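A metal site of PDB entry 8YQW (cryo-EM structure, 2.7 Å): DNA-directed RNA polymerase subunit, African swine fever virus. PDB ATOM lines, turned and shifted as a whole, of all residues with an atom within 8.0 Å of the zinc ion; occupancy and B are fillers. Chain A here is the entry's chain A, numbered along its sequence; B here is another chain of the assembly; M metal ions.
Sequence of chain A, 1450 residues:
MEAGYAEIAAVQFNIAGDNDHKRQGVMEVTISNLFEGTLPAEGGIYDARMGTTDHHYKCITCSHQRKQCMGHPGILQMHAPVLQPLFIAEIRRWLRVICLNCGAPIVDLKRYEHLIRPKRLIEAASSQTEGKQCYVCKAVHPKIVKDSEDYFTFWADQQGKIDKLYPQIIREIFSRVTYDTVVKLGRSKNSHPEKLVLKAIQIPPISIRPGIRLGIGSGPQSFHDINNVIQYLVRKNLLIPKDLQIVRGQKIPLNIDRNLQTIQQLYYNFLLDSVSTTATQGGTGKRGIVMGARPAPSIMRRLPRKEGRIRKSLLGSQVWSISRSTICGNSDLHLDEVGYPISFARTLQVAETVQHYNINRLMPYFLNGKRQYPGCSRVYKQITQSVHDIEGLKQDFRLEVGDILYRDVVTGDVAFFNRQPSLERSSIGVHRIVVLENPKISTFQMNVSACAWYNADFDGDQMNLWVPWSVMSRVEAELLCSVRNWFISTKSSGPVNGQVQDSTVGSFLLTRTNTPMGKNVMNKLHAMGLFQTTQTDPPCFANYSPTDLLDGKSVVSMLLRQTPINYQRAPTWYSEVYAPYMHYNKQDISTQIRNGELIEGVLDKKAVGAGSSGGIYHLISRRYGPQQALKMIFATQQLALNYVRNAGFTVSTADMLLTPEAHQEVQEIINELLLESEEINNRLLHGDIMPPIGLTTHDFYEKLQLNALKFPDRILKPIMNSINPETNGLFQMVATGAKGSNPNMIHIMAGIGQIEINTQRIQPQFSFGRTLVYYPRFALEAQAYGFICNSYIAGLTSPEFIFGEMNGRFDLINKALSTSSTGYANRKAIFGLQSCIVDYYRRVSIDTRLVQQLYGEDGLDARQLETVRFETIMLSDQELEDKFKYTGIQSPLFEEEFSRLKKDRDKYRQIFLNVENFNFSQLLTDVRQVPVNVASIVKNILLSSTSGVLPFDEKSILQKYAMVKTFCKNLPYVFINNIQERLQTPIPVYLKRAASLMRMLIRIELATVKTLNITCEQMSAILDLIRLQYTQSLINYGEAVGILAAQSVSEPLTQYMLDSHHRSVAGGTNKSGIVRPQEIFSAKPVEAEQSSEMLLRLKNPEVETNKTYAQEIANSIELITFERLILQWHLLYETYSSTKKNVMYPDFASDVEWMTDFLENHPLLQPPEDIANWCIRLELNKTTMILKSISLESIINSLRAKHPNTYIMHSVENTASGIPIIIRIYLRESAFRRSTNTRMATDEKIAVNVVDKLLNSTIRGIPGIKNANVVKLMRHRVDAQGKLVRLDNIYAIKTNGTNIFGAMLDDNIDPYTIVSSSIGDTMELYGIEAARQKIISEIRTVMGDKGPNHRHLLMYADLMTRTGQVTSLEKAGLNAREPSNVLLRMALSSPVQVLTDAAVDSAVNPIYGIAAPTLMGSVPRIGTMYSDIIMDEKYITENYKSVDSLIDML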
ATOM      1  N   ILE A  98     -23.929   8.780 -14.779  1.00  0.00           N
ATOM      2  CA  ILE A  98     -23.486   7.502 -15.298  1.00  0.00           C
ATOM      3  C   ILE A  98     -22.219   7.698 -16.113  1.00  0.00           C
ATOM      4  O   ILE A  98     -21.923   8.786 -16.612  1.00  0.00           O
ATOM      5  CB  ILE A  98     -24.579   6.822 -16.144  1.00  0.00           C
ATOM      6  CG1 ILE A  98     -24.838   7.639 -17.404  1.00  0.00           C
ATOM      7  CG2 ILE A  98     -25.856   6.663 -15.343  1.00  0.00           C
ATOM      8  CD1 ILE A  98     -25.746   6.975 -18.379  1.00  0.00           C
ATOM      9  N   CYS A  99     -21.451   6.622 -16.238  1.00  0.00           N
ATOM     10  CA  CYS A  99     -20.292   6.640 -17.129  1.00  0.00           C
ATOM     11  C   CYS A  99     -20.745   6.582 -18.581  1.00  0.00           C
ATOM     12  O   CYS A  99     -21.639   5.815 -18.937  1.00  0.00           O
ATOM     13  CB  CYS A  99     -19.377   5.466 -16.813  1.00  0.00           C
ATOM     14  SG  CYS A  99     -17.922   5.364 -17.883  1.00  0.00           S
ATOM     15  N   LEU A 100     -20.109   7.396 -19.423  1.00  0.00           N
ATOM     16  CA  LEU A 100     -20.470   7.491 -20.825  1.00  0.00           C
ATOM     17  C   LEU A 100     -19.866   6.377 -21.670  1.00  0.00           C
ATOM     18  O   LEU A 100     -20.082   6.371 -22.888  1.00  0.00           O
ATOM     19  CB  LEU A 100     -20.044   8.849 -21.391  1.00  0.00           C
ATOM     20  CG  LEU A 100     -21.063   9.982 -21.329  1.00  0.00           C
ATOM     21  CD1 LEU A 100     -21.415  10.331 -19.899  1.00  0.00           C
ATOM     22  CD2 LEU A 100     -20.532  11.199 -22.062  1.00  0.00           C
ATOM     23  N   ASN A 101     -19.125   5.450 -21.070  1.00  0.00           N
ATOM     24  CA  ASN A 101     -18.450   4.408 -21.834  1.00  0.00           C
ATOM     25  C   ASN A 101     -18.851   2.993 -21.427  1.00  0.00           C
ATOM     26  O   ASN A 101     -18.810   2.101 -22.281  1.00  0.00           O
ATOM     27  CB  ASN A 101     -16.925   4.551 -21.687  1.00  0.00           C
ATOM     28  CG  ASN A 101     -16.170   3.850 -22.806  1.00  0.00           C
ATOM     29  OD1 ASN A 101     -16.764   3.305 -23.731  1.00  0.00           O
ATOM     30  ND2 ASN A 101     -14.840   3.885 -22.731  1.00  0.00           N
ATOM     31  N   CYS A 102     -19.235   2.758 -20.168  1.00  0.00           N
ATOM     32  CA  CYS A 102     -19.668   1.441 -19.747  1.00  0.00           C
ATOM     33  C   CYS A 102     -21.047   1.426 -19.102  1.00  0.00           C
ATOM     34  O   CYS A 102     -21.582   0.336 -18.879  1.00  0.00           O
ATOM     35  CB  CYS A 102     -18.659   0.829 -18.767  1.00  0.00           C
ATOM     36  SG  CYS A 102     -18.586   1.655 -17.174  1.00  0.00           S
ATOM     37  N   GLY A 103     -21.626   2.580 -18.786  1.00  0.00           N
ATOM     38  CA  GLY A 103     -22.953   2.638 -18.210  1.00  0.00           C
ATOM     39  C   GLY A 103     -23.018   2.500 -16.710  1.00  0.00           C
ATOM     40  O   GLY A 103     -24.104   2.626 -16.141  1.00  0.00           O
ATOM     41  N   ALA A 104     -21.900   2.239 -16.055  1.00  0.00           N
ATOM     42  CA  ALA A 104     -21.887   2.110 -14.609  1.00  0.00           C
ATOM     43  C   ALA A 104     -21.993   3.474 -13.940  1.00  0.00           C
ATOM     44  O   ALA A 104     -21.636   4.493 -14.538  1.00  0.00           O
ATOM     45  CB  ALA A 104     -20.609   1.410 -14.154  1.00  0.00           C
ATOM     46  N   PRO A 105     -22.497   3.539 -12.716  1.00  0.00           N
ATOM     47  CA  PRO A 105     -22.573   4.824 -12.016  1.00  0.00           C
ATOM     48  C   PRO A 105     -21.189   5.333 -11.640  1.00  0.00           C
ATOM     49  O   PRO A 105     -20.248   4.566 -11.428  1.00  0.00           O
ATOM     50  CB  PRO A 105     -23.399   4.502 -10.760  1.00  0.00           C
ATOM     51  CG  PRO A 105     -23.177   3.054 -10.544  1.00  0.00           C
ATOM     52  CD  PRO A 105     -23.059   2.435 -11.899  1.00  0.00           C
ATOM     53  N   ILE A 106     -21.079   6.650 -11.557  1.00  0.00           N
ATOM     54  CA  ILE A 106     -19.851   7.317 -11.130  1.00  0.00           C
ATOM     55  C   ILE A 106     -19.948   7.767  -9.687  1.00  0.00           C
ATOM     56  O   ILE A 106     -19.026   7.545  -8.894  1.00  0.00           O
ATOM     57  CB  ILE A 106     -19.529   8.504 -12.063  1.00  0.00           C
ATOM     58  CG1 ILE A 106     -19.192   7.998 -13.465  1.00  0.00           C
ATOM     59  CG2 ILE A 106     -18.378   9.313 -11.511  1.00  0.00           C
ATOM     60  CD1 ILE A 106     -19.318   9.048 -14.521  1.00  0.00           C
ATOM     61  N   GLN A 133     -13.086   9.400 -12.158  1.00  0.00           N
ATOM     62  CA  GLN A 133     -12.571   8.188 -12.775  1.00  0.00           C
ATOM     63  C   GLN A 133     -13.520   7.032 -12.520  1.00  0.00           C
ATOM     64  O   GLN A 133     -14.006   6.853 -11.394  1.00  0.00           O
ATOM     65  CB  GLN A 133     -11.174   7.851 -12.232  1.00  0.00           C
ATOM     66  CG  GLN A 133     -10.523   6.658 -12.916  1.00  0.00           C
ATOM     67  CD  GLN A 133     -10.274   6.897 -14.385  1.00  0.00           C
ATOM     68  OE1 GLN A 133     -10.977   6.354 -15.239  1.00  0.00           O
ATOM     69  NE2 GLN A 133      -9.284   7.719 -14.702  1.00  0.00           N
ATOM     70  N   CYS A 134     -13.801   6.254 -13.558  1.00  0.00           N
ATOM     71  CA  CYS A 134     -14.689   5.115 -13.436  1.00  0.00           C
ATOM     72  C   CYS A 134     -13.983   3.962 -12.717  1.00  0.00           C
ATOM     73  O   CYS A 134     -12.763   3.808 -12.799  1.00  0.00           O
ATOM     74  CB  CYS A 134     -15.173   4.661 -14.811  1.00  0.00           C
ATOM     75  SG  CYS A 134     -16.568   3.524 -14.761  1.00  0.00           S
ATOM     76  N   TYR A 135     -14.772   3.151 -12.022  1.00  0.00           N
ATOM     77  CA  TYR A 135     -14.238   2.047 -11.242  1.00  0.00           C
ATOM     78  C   TYR A 135     -14.197   0.722 -11.993  1.00  0.00           C
ATOM     79  O   TYR A 135     -13.607  -0.238 -11.493  1.00  0.00           O
ATOM     80  CB  TYR A 135     -15.052   1.862  -9.954  1.00  0.00           C
ATOM     81  CG  TYR A 135     -14.855   2.965  -8.937  1.00  0.00           C
ATOM     82  CD1 TYR A 135     -15.485   4.189  -9.079  1.00  0.00           C
ATOM     83  CD2 TYR A 135     -14.037   2.777  -7.827  1.00  0.00           C
ATOM     84  CE1 TYR A 135     -15.302   5.199  -8.145  1.00  0.00           C
ATOM     85  CE2 TYR A 135     -13.852   3.775  -6.899  1.00  0.00           C
ATOM     86  CZ  TYR A 135     -14.491   4.990  -7.059  1.00  0.00           C
ATOM     87  OH  TYR A 135     -14.308   5.997  -6.135  1.00  0.00           O
ATOM     88  N   VAL A 136     -14.813   0.634 -13.171  1.00  0.00           N
ATOM     89  CA  VAL A 136     -14.905  -0.637 -13.872  1.00  0.00           C
ATOM     90  C   VAL A 136     -14.387  -0.582 -15.303  1.00  0.00           C
ATOM     91  O   VAL A 136     -14.036  -1.642 -15.856  1.00  0.00           O
ATOM     92  CB  VAL A 136     -16.357  -1.162 -13.858  1.00  0.00           C
ATOM     93  CG1 VAL A 136     -16.744  -1.628 -12.456  1.00  0.00           C
ATOM     94  CG2 VAL A 136     -17.307  -0.095 -14.337  1.00  0.00           C
ATOM     95  N   CYS A 137     -14.321   0.580 -15.946  1.00  0.00           N
ATOM     96  CA  CYS A 137     -13.808   0.673 -17.306  1.00  0.00           C
ATOM     97  C   CYS A 137     -12.646   1.636 -17.457  1.00  0.00           C
ATOM     98  O   CYS A 137     -12.061   1.700 -18.546  1.00  0.00           O
ATOM     99  CB  CYS A 137     -14.928   1.095 -18.280  1.00  0.00           C
ATOM    100  SG  CYS A 137     -15.184   2.871 -18.345  1.00  0.00           S
ATOM    101  N   LYS A 138     -12.298   2.391 -16.408  1.00  0.00           N
ATOM    102  CA  LYS A 138     -11.170   3.314 -16.416  1.00  0.00           C
ATOM    103  C   LYS A 138     -11.319   4.360 -17.525  1.00  0.00           C
ATOM    104  O   LYS A 138     -10.520   4.424 -18.467  1.00  0.00           O
ATOM    105  CB  LYS A 138      -9.847   2.552 -16.536  1.00  0.00           C
ATOM    106  CG  LYS A 138      -9.712   1.396 -15.557  1.00  0.00           C
ATOM    107  CD  LYS A 138      -9.455   1.911 -14.138  1.00  0.00           C
ATOM    108  CE  LYS A 138      -9.466   0.768 -13.148  1.00  0.00           C
ATOM    109  NZ  LYS A 138      -8.407  -0.235 -13.463  1.00  0.00           N
ATOM    110  N   ALA A 139     -12.355   5.174 -17.393  1.00  0.00           N
ATOM    111  CA  ALA A 139     -12.591   6.292 -18.297  1.00  0.00           C
ATOM    112  C   ALA A 139     -12.821   7.560 -17.488  1.00  0.00           C
ATOM    113  O   ALA A 139     -13.446   7.528 -16.434  1.00  0.00           O
ATOM    114  CB  ALA A 139     -13.801   6.033 -19.204  1.00  0.00           C
ATOM    115  N   VAL A 140     -12.295   8.671 -17.987  1.00  0.00           N
ATOM    116  CA  VAL A 140     -12.447   9.963 -17.334  1.00  0.00           C
ATOM    117  C   VAL A 140     -13.765  10.573 -17.767  1.00  0.00           C
ATOM    118  O   VAL A 140     -14.004  10.766 -18.966  1.00  0.00           O
ATOM    119  CB  VAL A 140     -11.268  10.897 -17.678  1.00  0.00           C
ATOM    120  CG1 VAL A 140     -11.381  12.188 -16.885  1.00  0.00           C
ATOM    121  CG2 VAL A 140      -9.947  10.196 -17.393  1.00  0.00           C
ATOM    122  N   HIS A 141     -14.614  10.881 -16.799  1.00  0.00           N
ATOM    123  CA  HIS A 141     -15.933  11.432 -17.101  1.00  0.00           C
ATOM    124  C   HIS A 141     -15.798  12.878 -17.572  1.00  0.00           C
ATOM    125  O   HIS A 141     -15.246  13.700 -16.842  1.00  0.00           O
ATOM    126  CB  HIS A 141     -16.839  11.364 -15.882  1.00  0.00           C
ATOM    127  CG  HIS A 141     -18.232  11.848 -16.139  1.00  0.00           C
ATOM    128  ND1 HIS A 141     -19.083  11.225 -17.021  1.00  0.00           N
ATOM    129  CD2 HIS A 141     -18.914  12.906 -15.640  1.00  0.00           C
ATOM    130  CE1 HIS A 141     -20.235  11.872 -17.044  1.00  0.00           C
ATOM    131  NE2 HIS A 141     -20.162  12.892 -16.214  1.00  0.00           N
ATOM    132  N   ARG A 176     -27.142   1.316 -21.747  1.00  0.00           N
ATOM    133  CA  ARG A 176     -26.131   0.590 -21.001  1.00  0.00           C
ATOM    134  C   ARG A 176     -26.322   0.700 -19.494  1.00  0.00           C
ATOM    135  O   ARG A 176     -25.506   0.161 -18.741  1.00  0.00           O
ATOM    136  CB  ARG A 176     -24.749   1.103 -21.421  1.00  0.00           C
ATOM    137  CG  ARG A 176     -23.661   0.057 -21.364  1.00  0.00           C
ATOM    138  CD  ARG A 176     -22.368   0.548 -22.004  1.00  0.00           C
ATOM    139  NE  ARG A 176     -22.523   0.914 -23.407  1.00  0.00           N
ATOM    140  CZ  ARG A 176     -22.210   2.107 -23.902  1.00  0.00           C
ATOM    141  NH1 ARG A 176     -21.750   3.075 -23.136  1.00  0.00           N
ATOM    142  NH2 ARG A 176     -22.367   2.320 -25.214  1.00  0.00           N
ATOM    143  N   LEU B 117     -23.273  -5.241 -15.602  1.00  0.00           N
ATOM    144  CA  LEU B 117     -23.309  -4.160 -16.581  1.00  0.00           C
ATOM    145  C   LEU B 117     -24.293  -4.516 -17.679  1.00  0.00           C
ATOM    146  O   LEU B 117     -24.510  -5.683 -17.984  1.00  0.00           O
ATOM    147  CB  LEU B 117     -21.925  -3.886 -17.187  1.00  0.00           C
ATOM    148  CG  LEU B 117     -20.979  -2.903 -16.485  1.00  0.00           C
ATOM    149  CD1 LEU B 117     -20.299  -3.556 -15.296  1.00  0.00           C
ATOM    150  CD2 LEU B 117     -19.950  -2.366 -17.463  1.00  0.00           C
HETATM  151 ZN    ZN M   1     -17.037   3.391 -17.033  1.00  0.00          ZN
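The side-chain sulfur of Cys 99 lies close to the backbone NH of Asn 101 (3.4 Å).
The backbone NH of Cys 99 lies within hydrogen-bond range of the backbone carbonyl oxygen of Ala 104, 2.7 Å away.
SG of Cys 134 sits close to N of Val 136, 3.7 Å away.
O of Ala 139 lies within hydrogen-bond range of N of Cys 134, at 3.2 Å.
The side-chain sulfur (SG) of Cys 137 sits close to the backbone NH (N) of Ala 139 (3.8 Å).
The backbone NH (N) of Ala 104 sits close to the side-chain sulfur (SG) of Cys 102 (3.5 Å).
Within 4 Å of the zinc ion: Cys 99, Cys 102, Cys 134 and Cys 137.
The nearest printed residue that does not touch the zinc ion is Val 136 (4.4 Å).
SG of Cys 99 is bound to the zinc ion, at 2.3 Å.
SG of Cys 134 is bound to the zinc ion (2.3 Å).
The zinc ion is bound by SG of Cys 137.
The zinc ion is bound by the side-chain sulfur (SG) of Cys 102.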
